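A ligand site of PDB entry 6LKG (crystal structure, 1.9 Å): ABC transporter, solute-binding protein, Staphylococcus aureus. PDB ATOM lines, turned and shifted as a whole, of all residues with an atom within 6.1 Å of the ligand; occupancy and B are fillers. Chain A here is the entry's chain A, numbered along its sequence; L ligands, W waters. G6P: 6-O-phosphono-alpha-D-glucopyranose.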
ATOM      1  N   SER A   7       0.822 -15.866  24.224  1.00  0.00           N
ATOM      2  CA  SER A   7       1.495 -15.131  23.160  1.00  0.00           C
ATOM      3  C   SER A   7       2.734 -14.385  23.638  1.00  0.00           C
ATOM      4  O   SER A   7       2.674 -13.647  24.626  1.00  0.00           O
ATOM      5  CB  SER A   7       0.541 -14.131  22.506  1.00  0.00           C
ATOM      6  OG  SER A   7       1.158 -13.497  21.407  1.00  0.00           O
ATOM      7  N   PRO A   8       3.874 -14.549  22.956  1.00  0.00           N
ATOM      8  CA  PRO A   8       5.035 -13.694  23.242  1.00  0.00           C
ATOM      9  C   PRO A   8       4.967 -12.334  22.565  1.00  0.00           C
ATOM     10  O   PRO A   8       5.841 -11.507  22.798  1.00  0.00           O
ATOM     11  CB  PRO A   8       6.201 -14.520  22.689  1.00  0.00           C
ATOM     12  CG  PRO A   8       5.597 -15.310  21.574  1.00  0.00           C
ATOM     13  CD  PRO A   8       4.187 -15.624  21.999  1.00  0.00           C
ATOM     14  N   TYR A   9       3.951 -12.089  21.727  1.00  0.00           N
ATOM     15  CA  TYR A   9       3.805 -10.800  21.066  1.00  0.00           C
ATOM     16  C   TYR A   9       3.597  -9.697  22.101  1.00  0.00           C
ATOM     17  O   TYR A   9       3.044  -9.918  23.179  1.00  0.00           O
ATOM     18  CB  TYR A   9       2.614 -10.824  20.114  1.00  0.00           C
ATOM     19  CG  TYR A   9       2.857 -11.516  18.801  1.00  0.00           C
ATOM     20  CD1 TYR A   9       3.976 -11.216  18.025  1.00  0.00           C
ATOM     21  CD2 TYR A   9       1.965 -12.459  18.314  1.00  0.00           C
ATOM     22  CE1 TYR A   9       4.185 -11.844  16.813  1.00  0.00           C
ATOM     23  CE2 TYR A   9       2.161 -13.092  17.107  1.00  0.00           C
ATOM     24  CZ  TYR A   9       3.283 -12.789  16.362  1.00  0.00           C
ATOM     25  OH  TYR A   9       3.495 -13.417  15.160  1.00  0.00           O
ATOM     26  N   GLN A  10       4.049  -8.501  21.746  1.00  0.00           N
ATOM     27  CA  GLN A  10       3.713  -7.327  22.544  1.00  0.00           C
ATOM     28  C   GLN A  10       2.224  -7.046  22.431  1.00  0.00           C
ATOM     29  O   GLN A  10       1.598  -7.269  21.387  1.00  0.00           O
ATOM     30  CB  GLN A  10       4.519  -6.111  22.088  1.00  0.00           C
ATOM     31  CG  GLN A  10       5.980  -6.130  22.541  1.00  0.00           C
ATOM     32  CD  GLN A  10       6.123  -6.081  24.050  1.00  0.00           C
ATOM     33  OE1 GLN A  10       6.259  -7.118  24.713  1.00  0.00           O
ATOM     34  NE2 GLN A  10       6.116  -4.882  24.617  1.00  0.00           N
ATOM     35  N   GLY A  34       4.627 -13.504  27.744  1.00  0.00           N
ATOM     36  CA  GLY A  34       5.867 -14.017  28.296  1.00  0.00           C
ATOM     37  C   GLY A  34       6.787 -14.453  27.175  1.00  0.00           C
ATOM     38  O   GLY A  34       6.403 -14.495  26.014  1.00  0.00           O
ATOM     39  N   SER A  35       8.010 -14.783  27.558  1.00  0.00           N
ATOM     40  CA  SER A  35       8.945 -15.327  26.588  1.00  0.00           C
ATOM     41  C   SER A  35       8.372 -16.612  26.001  1.00  0.00           C
ATOM     42  O   SER A  35       7.634 -17.352  26.661  1.00  0.00           O
ATOM     43  CB  SER A  35      10.299 -15.567  27.245  1.00  0.00           C
ATOM     44  OG  SER A  35      10.798 -14.370  27.824  1.00  0.00           O
ATOM     45  N   THR A  36       8.721 -16.868  24.738  1.00  0.00           N
ATOM     46  CA  THR A  36       8.109 -17.978  24.001  1.00  0.00           C
ATOM     47  C   THR A  36       8.304 -19.300  24.739  1.00  0.00           C
ATOM     48  O   THR A  36       7.341 -20.026  24.992  1.00  0.00           O
ATOM     49  CB  THR A  36       8.688 -18.073  22.593  1.00  0.00           C
ATOM     50  OG1 THR A  36       8.442 -16.845  21.882  1.00  0.00           O
ATOM     51  CG2 THR A  36       8.053 -19.232  21.831  1.00  0.00           C
ATOM     52  N   GLN A  37       9.546 -19.633  25.082  1.00  0.00           N
ATOM     53  CA  GLN A  37       9.817 -20.929  25.706  1.00  0.00           C
ATOM     54  C   GLN A  37       9.330 -20.975  27.140  1.00  0.00           C
ATOM     55  O   GLN A  37       9.012 -22.055  27.651  1.00  0.00           O
ATOM     56  CB  GLN A  37      11.309 -21.240  25.625  1.00  0.00           C
ATOM     57  CG  GLN A  37      11.826 -21.428  24.215  1.00  0.00           C
ATOM     58  CD  GLN A  37      11.096 -22.529  23.469  1.00  0.00           C
ATOM     59  OE1 GLN A  37      10.842 -23.602  24.010  1.00  0.00           O
ATOM     60  NE2 GLN A  37      10.739 -22.263  22.212  1.00  0.00           N
ATOM     61  N   MET A  56      -0.171 -18.188  19.922  1.00  0.00           N
ATOM     62  CA  MET A  56       0.153 -17.408  18.735  1.00  0.00           C
ATOM     63  C   MET A  56       1.431 -16.623  18.985  1.00  0.00           C
ATOM     64  O   MET A  56       1.587 -16.000  20.038  1.00  0.00           O
ATOM     65  CB  MET A  56      -0.996 -16.469  18.334  1.00  0.00           C
ATOM     66  CG  MET A  56      -1.367 -15.414  19.354  1.00  0.00           C
ATOM     67  SD  MET A  56      -2.715 -14.350  18.797  1.00  0.00           S
ATOM     68  CE  MET A  56      -1.978 -13.589  17.347  1.00  0.00           C
ATOM     69  N   GLY A  57       2.339 -16.652  18.021  1.00  0.00           N
ATOM     70  CA  GLY A  57       3.622 -15.998  18.158  1.00  0.00           C
ATOM     71  C   GLY A  57       4.749 -16.984  18.384  1.00  0.00           C
ATOM     72  O   GLY A  57       4.555 -18.105  18.869  1.00  0.00           O
ATOM     73  N   GLY A  58       5.950 -16.551  18.031  1.00  0.00           N
ATOM     74  CA  GLY A  58       7.116 -17.402  18.086  1.00  0.00           C
ATOM     75  C   GLY A  58       7.204 -18.339  16.888  1.00  0.00           C
ATOM     76  O   GLY A  58       6.250 -18.544  16.140  1.00  0.00           O
ATOM     77  N   VAL A  59       8.389 -18.919  16.721  1.00  0.00           N
ATOM     78  CA  VAL A  59       8.627 -19.845  15.616  1.00  0.00           C
ATOM     79  C   VAL A  59       8.165 -21.240  16.032  1.00  0.00           C
ATOM     80  O   VAL A  59       8.982 -22.136  16.260  1.00  0.00           O
ATOM     81  CB  VAL A  59      10.108 -19.845  15.185  1.00  0.00           C
ATOM     82  CG1 VAL A  59      10.398 -18.610  14.337  1.00  0.00           C
ATOM     83  CG2 VAL A  59      11.025 -19.855  16.400  1.00  0.00           C
ATOM     84  N   MET A  98       8.462 -12.512  10.290  1.00  0.00           N
ATOM     85  CA  MET A  98       9.099 -11.546  11.194  1.00  0.00           C
ATOM     86  C   MET A  98      10.613 -11.608  11.049  1.00  0.00           C
ATOM     87  O   MET A  98      11.257 -12.519  11.619  1.00  0.00           O
ATOM     88  CB  MET A  98       8.689 -11.815  12.634  1.00  0.00           C
ATOM     89  CG  MET A  98       9.167 -10.752  13.612  1.00  0.00           C
ATOM     90  SD  MET A  98       8.283  -9.199  13.399  1.00  0.00           S
ATOM     91  CE  MET A  98       6.639  -9.690  13.917  1.00  0.00           C
ATOM     92  N   PRO A  99      11.228 -10.674  10.334  1.00  0.00           N
ATOM     93  CA  PRO A  99      12.689 -10.657  10.254  1.00  0.00           C
ATOM     94  C   PRO A  99      13.305 -10.296  11.606  1.00  0.00           C
ATOM     95  O   PRO A  99      12.847  -9.391  12.301  1.00  0.00           O
ATOM     96  CB  PRO A  99      12.978  -9.573   9.209  1.00  0.00           C
ATOM     97  CG  PRO A  99      11.689  -9.362   8.483  1.00  0.00           C
ATOM     98  CD  PRO A  99      10.610  -9.637   9.480  1.00  0.00           C
ATOM     99  N   THR A 100      14.348 -11.045  11.968  1.00  0.00           N
ATOM    100  CA  THR A 100      15.177 -10.659  13.101  1.00  0.00           C
ATOM    101  C   THR A 100      16.195  -9.618  12.656  1.00  0.00           C
ATOM    102  O   THR A 100      16.707  -9.673  11.541  1.00  0.00           O
ATOM    103  CB  THR A 100      15.889 -11.888  13.689  1.00  0.00           C
ATOM    104  OG1 THR A 100      16.675 -12.515  12.666  1.00  0.00           O
ATOM    105  CG2 THR A 100      14.874 -12.883  14.231  1.00  0.00           C
ATOM    106  N   SER A 132      18.735 -11.181  24.135  1.00  0.00           N
ATOM    107  CA  SER A 132      17.858 -11.884  25.062  1.00  0.00           C
ATOM    108  C   SER A 132      18.250 -13.356  25.164  1.00  0.00           C
ATOM    109  O   SER A 132      18.861 -13.928  24.262  1.00  0.00           O
ATOM    110  CB  SER A 132      16.396 -11.750  24.635  1.00  0.00           C
ATOM    111  OG  SER A 132      16.227 -12.058  23.255  1.00  0.00           O
ATOM    112  N   THR A 136      15.182 -19.160  26.543  1.00  0.00           N
ATOM    113  CA  THR A 136      13.802 -18.867  26.871  1.00  0.00           C
ATOM    114  C   THR A 136      13.047 -18.061  25.825  1.00  0.00           C
ATOM    115  O   THR A 136      11.815 -17.984  25.907  1.00  0.00           O
ATOM    116  CB  THR A 136      13.730 -18.096  28.207  1.00  0.00           C
ATOM    117  OG1 THR A 136      14.474 -16.878  28.106  1.00  0.00           O
ATOM    118  CG2 THR A 136      14.304 -18.949  29.341  1.00  0.00           C
ATOM    119  N   THR A 137      13.730 -17.476  24.838  1.00  0.00           N
ATOM    120  CA  THR A 137      13.100 -16.571  23.887  1.00  0.00           C
ATOM    121  C   THR A 137      13.249 -17.079  22.456  1.00  0.00           C
ATOM    122  O   THR A 137      14.206 -17.787  22.124  1.00  0.00           O
ATOM    123  CB  THR A 137      13.704 -15.161  23.963  1.00  0.00           C
ATOM    124  OG1 THR A 137      15.057 -15.185  23.484  1.00  0.00           O
ATOM    125  CG2 THR A 137      13.670 -14.630  25.384  1.00  0.00           C
ATOM    126  N   THR A 138      12.283 -16.713  21.614  1.00  0.00           N
ATOM    127  CA  THR A 138      12.416 -16.958  20.186  1.00  0.00           C
ATOM    128  C   THR A 138      13.524 -16.105  19.583  1.00  0.00           C
ATOM    129  O   THR A 138      14.334 -16.587  18.791  1.00  0.00           O
ATOM    130  CB  THR A 138      11.095 -16.676  19.465  1.00  0.00           C
ATOM    131  OG1 THR A 138      10.137 -17.682  19.803  1.00  0.00           O
ATOM    132  CG2 THR A 138      11.295 -16.672  17.967  1.00  0.00           C
ATOM    133  N   THR A 139      13.585 -14.820  19.967  1.00  0.00           N
ATOM    134  CA  THR A 139      14.491 -13.880  19.314  1.00  0.00           C
ATOM    135  C   THR A 139      15.941 -14.229  19.601  1.00  0.00           C
ATOM    136  O   THR A 139      16.772 -14.282  18.686  1.00  0.00           O
ATOM    137  CB  THR A 139      14.176 -12.453  19.770  1.00  0.00           C
ATOM    138  OG1 THR A 139      12.804 -12.162  19.485  1.00  0.00           O
ATOM    139  CG2 THR A 139      15.067 -11.461  19.039  1.00  0.00           C
ATOM    140  N   GLY A 140      16.280 -14.473  20.876  1.00  0.00           N
ATOM    141  CA  GLY A 140      17.641 -14.841  21.205  1.00  0.00           C
ATOM    142  C   GLY A 140      18.070 -16.137  20.561  1.00  0.00           C
ATOM    143  O   GLY A 140      19.206 -16.268  20.096  1.00  0.00           O
ATOM    144  N   LYS A 169      14.460 -10.506  28.925  1.00  0.00           N
ATOM    145  CA  LYS A 169      13.310 -10.246  28.063  1.00  0.00           C
ATOM    146  C   LYS A 169      13.757  -9.654  26.738  1.00  0.00           C
ATOM    147  O   LYS A 169      14.601  -8.751  26.707  1.00  0.00           O
ATOM    148  CB  LYS A 169      12.313  -9.312  28.749  1.00  0.00           C
ATOM    149  CG  LYS A 169      11.813  -9.820  30.097  1.00  0.00           C
ATOM    150  CD  LYS A 169      11.026 -11.111  29.944  1.00  0.00           C
ATOM    151  CE  LYS A 169       9.718 -10.881  29.205  1.00  0.00           C
ATOM    152  NZ  LYS A 169       8.861 -12.105  29.209  1.00  0.00           N
ATOM    153  N   THR A 170      13.173 -10.149  25.648  1.00  0.00           N
ATOM    154  CA  THR A 170      13.517  -9.642  24.327  1.00  0.00           C
ATOM    155  C   THR A 170      13.192  -8.160  24.200  1.00  0.00           C
ATOM    156  O   THR A 170      13.996  -7.376  23.677  1.00  0.00           O
ATOM    157  CB  THR A 170      12.776 -10.441  23.243  1.00  0.00           C
ATOM    158  OG1 THR A 170      13.304 -11.765  23.191  1.00  0.00           O
ATOM    159  CG2 THR A 170      12.934  -9.775  21.879  1.00  0.00           C
ATOM    160  N   SER A 171      12.027  -7.730  24.708  1.00  0.00           N
ATOM    161  CA  SER A 171      11.635  -6.338  24.592  1.00  0.00           C
ATOM    162  C   SER A 171      12.484  -5.420  25.458  1.00  0.00           C
ATOM    163  O   SER A 171      12.513  -4.200  25.210  1.00  0.00           O
ATOM    164  CB  SER A 171      10.158  -6.171  24.963  1.00  0.00           C
ATOM    165  OG  SER A 171       9.326  -6.686  23.933  1.00  0.00           O
ATOM    166  N   SER A 187      17.243  -7.828  18.170  1.00  0.00           N
ATOM    167  CA  SER A 187      15.805  -7.682  18.364  1.00  0.00           C
ATOM    168  C   SER A 187      15.081  -8.294  17.163  1.00  0.00           C
ATOM    169  O   SER A 187      15.641  -9.099  16.411  1.00  0.00           O
ATOM    170  CB  SER A 187      15.451  -6.203  18.591  1.00  0.00           C
ATOM    171  OG  SER A 187      14.075  -6.033  18.848  1.00  0.00           O
ATOM    172  N   TYR A 188      13.818  -7.918  16.978  1.00  0.00           N
ATOM    173  CA  TYR A 188      13.051  -8.316  15.811  1.00  0.00           C
ATOM    174  C   TYR A 188      12.347  -7.087  15.241  1.00  0.00           C
ATOM    175  O   TYR A 188      12.265  -6.034  15.874  1.00  0.00           O
ATOM    176  CB  TYR A 188      12.057  -9.442  16.126  1.00  0.00           C
ATOM    177  CG  TYR A 188      11.003  -9.133  17.165  1.00  0.00           C
ATOM    178  CD1 TYR A 188      11.281  -9.191  18.524  1.00  0.00           C
ATOM    179  CD2 TYR A 188       9.710  -8.803  16.787  1.00  0.00           C
ATOM    180  CE1 TYR A 188      10.318  -8.915  19.474  1.00  0.00           C
ATOM    181  CE2 TYR A 188       8.727  -8.531  17.724  1.00  0.00           C
ATOM    182  CZ  TYR A 188       9.035  -8.584  19.060  1.00  0.00           C
ATOM    183  OH  TYR A 188       8.061  -8.317  19.993  1.00  0.00           O
ATOM    184  N   ASN A 214      11.870 -15.196  10.795  1.00  0.00           N
ATOM    185  CA  ASN A 214      10.981 -15.973  11.639  1.00  0.00           C
ATOM    186  C   ASN A 214       9.661 -16.179  10.933  1.00  0.00           C
ATOM    187  O   ASN A 214       9.039 -15.209  10.462  1.00  0.00           O
ATOM    188  CB  ASN A 214      10.745 -15.269  12.982  1.00  0.00           C
ATOM    189  CG  ASN A 214      11.995 -15.188  13.828  1.00  0.00           C
ATOM    190  OD1 ASN A 214      13.035 -15.767  13.502  1.00  0.00           O
ATOM    191  ND2 ASN A 214      11.904 -14.463  14.935  1.00  0.00           N
ATOM    192  N   ASP A 216       6.346 -16.922  12.073  1.00  0.00           N
ATOM    193  CA  ASP A 216       5.525 -17.012  13.267  1.00  0.00           C
ATOM    194  C   ASP A 216       4.321 -17.909  13.018  1.00  0.00           C
ATOM    195  O   ASP A 216       3.753 -17.921  11.927  1.00  0.00           O
ATOM    196  CB  ASP A 216       5.065 -15.611  13.691  1.00  0.00           C
ATOM    197  CG  ASP A 216       6.205 -14.749  14.188  1.00  0.00           C
ATOM    198  OD1 ASP A 216       7.352 -15.242  14.263  1.00  0.00           O
ATOM    199  OD2 ASP A 216       5.962 -13.564  14.512  1.00  0.00           O
HETATM  200  C1  G6P L   1      10.262 -13.283  17.872  1.00  0.00           C
HETATM  201  C2  G6P L   1       8.991 -13.638  17.067  1.00  0.00           C
HETATM  202  C3  G6P L   1       7.729 -13.042  17.563  1.00  0.00           C
HETATM  203  C4  G6P L   1       7.683 -13.045  19.024  1.00  0.00           C
HETATM  204  C5  G6P L   1       8.776 -12.122  19.563  1.00  0.00           C
HETATM  205  C6  G6P L   1       8.759 -12.166  21.065  1.00  0.00           C
HETATM  206  O1  G6P L   1      11.174 -12.628  17.037  1.00  0.00           O
HETATM  207  O2  G6P L   1       9.177 -13.254  15.694  1.00  0.00           O
HETATM  208  O3  G6P L   1       6.582 -13.868  17.060  1.00  0.00           O
HETATM  209  O4  G6P L   1       6.390 -12.564  19.475  1.00  0.00           O
HETATM  210  O5  G6P L   1      10.135 -12.491  19.102  1.00  0.00           O
HETATM  211  O6  G6P L   1       9.034 -13.483  21.483  1.00  0.00           O
HETATM  212  P   G6P L   1      10.358 -13.757  22.503  1.00  0.00           P
HETATM  213  O1P G6P L   1      10.329 -15.216  22.947  1.00  0.00           O
HETATM  214  O2P G6P L   1      11.671 -13.464  21.772  1.00  0.00           O
HETATM  215  O3P G6P L   1      10.245 -12.896  23.709  1.00  0.00           O
HETATM  216  O   HOH W   1      11.113 -12.093  26.017  1.00  0.00           O
HETATM  217  O   HOH W   2       8.029 -11.428  24.295  1.00  0.00           O
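The side-chain carboxylate (OD2) of Asp 216 lies within hydrogen-bond range of an oxygen (O3) of the ligand, at 2.6 Å. The backbone NH (N) of Thr 36 sits at hydrogen-bond distance from an oxygen (O1P) of the ligand (2.9 Å). OG1 of Thr 36 sits at hydrogen-bond distance from O1P of the ligand (2.7 Å). N of Thr 139 sits at hydrogen-bond distance from O2P of the ligand (3.0 Å). The side-chain hydroxyl (OG1) of Thr 139 is in hydrogen-bond range of an oxygen (O5) of the ligand. The side-chain hydroxyl (OG1) of Thr 170 lies within hydrogen-bond range of an oxygen (O2P) of the ligand (2.8 Å). An oxygen (O1P) of the ligand sits at hydrogen-bond distance from the backbone NH (N) of Thr 138 (2.8 Å). The side-chain amide nitrogen (ND2) of Asn 214 is in hydrogen-bond range of an oxygen (O1) of the ligand (2.9 Å). O3 of the ligand lies within hydrogen-bond range of N of Gly 58 (2.9 Å). N of Tyr 9 lies close to O4 of the ligand.
The side-chain hydroxyl of Tyr 9 lies within hydrogen-bond range of the side-chain carboxylate of Asp 216 (2.6 Å). OG1 of Thr 36 is in hydrogen-bond range of OG1 of Thr 138, at 2.8 Å. OG1 of Thr 170 is in hydrogen-bond range of OG of Ser 132 (2.9 Å). The backbone carbonyl oxygen of Asn 214 lies within hydrogen-bond range of the backbone NH of Met 98 (2.8 Å). The backbone NH of Tyr 9 lies within hydrogen-bond range of the side-chain hydroxyl of Ser 7, 3.1 Å away. The backbone NH of Gly 140 is in hydrogen-bond range of the side-chain hydroxyl of Thr 137. OG1 of Thr 137 lies within hydrogen-bond range of OG of Ser 132 (3.3 Å). The side-chain hydroxyl (OG) of Ser 35 is in hydrogen-bond range of the side-chain amino group (NZ) of Lys 169, 3.3 Å away.
CB of Pro 8 touches O6 of the ligand, at 3.2 Å. C of Ser 35 touches O1P of the ligand (3.9 Å). CA of Gly 57 touches O3 of the ligand (3.8 Å). Met 98 touches the ligand. CA of Thr 137 touches O1P of the ligand, 3.2 Å away. Tyr 188 touches the ligand (CB to O1, 3.4 Å). Hydrophobic or aromatic side chains that line the ligand: Pro 8, Tyr 9, Met 98 and Tyr 188. 14 residues have an atom within 4 Å of the ligand: Pro 8, Tyr 9, Ser 35, Thr 36, Gly 57, Gly 58, Met 98, Thr 137, Thr 138, Thr 139, Thr 170, Tyr 188, Asn 214 and Asp 216. The nearest printed residue that does not touch the ligand is Thr 136 (4.3 Å).
Water W1 lies within hydrogen-bond range of an oxygen (O3P) of the ligand (2.6 Å), the backbone NH (N) of Thr 170 (2.9 Å) and the side-chain hydroxyl (OG) of Ser 35 (2.9 Å). Water W2 lies within hydrogen-bond range of O of Pro 8 (2.7 Å) and O3P of the ligand (2.7 Å).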
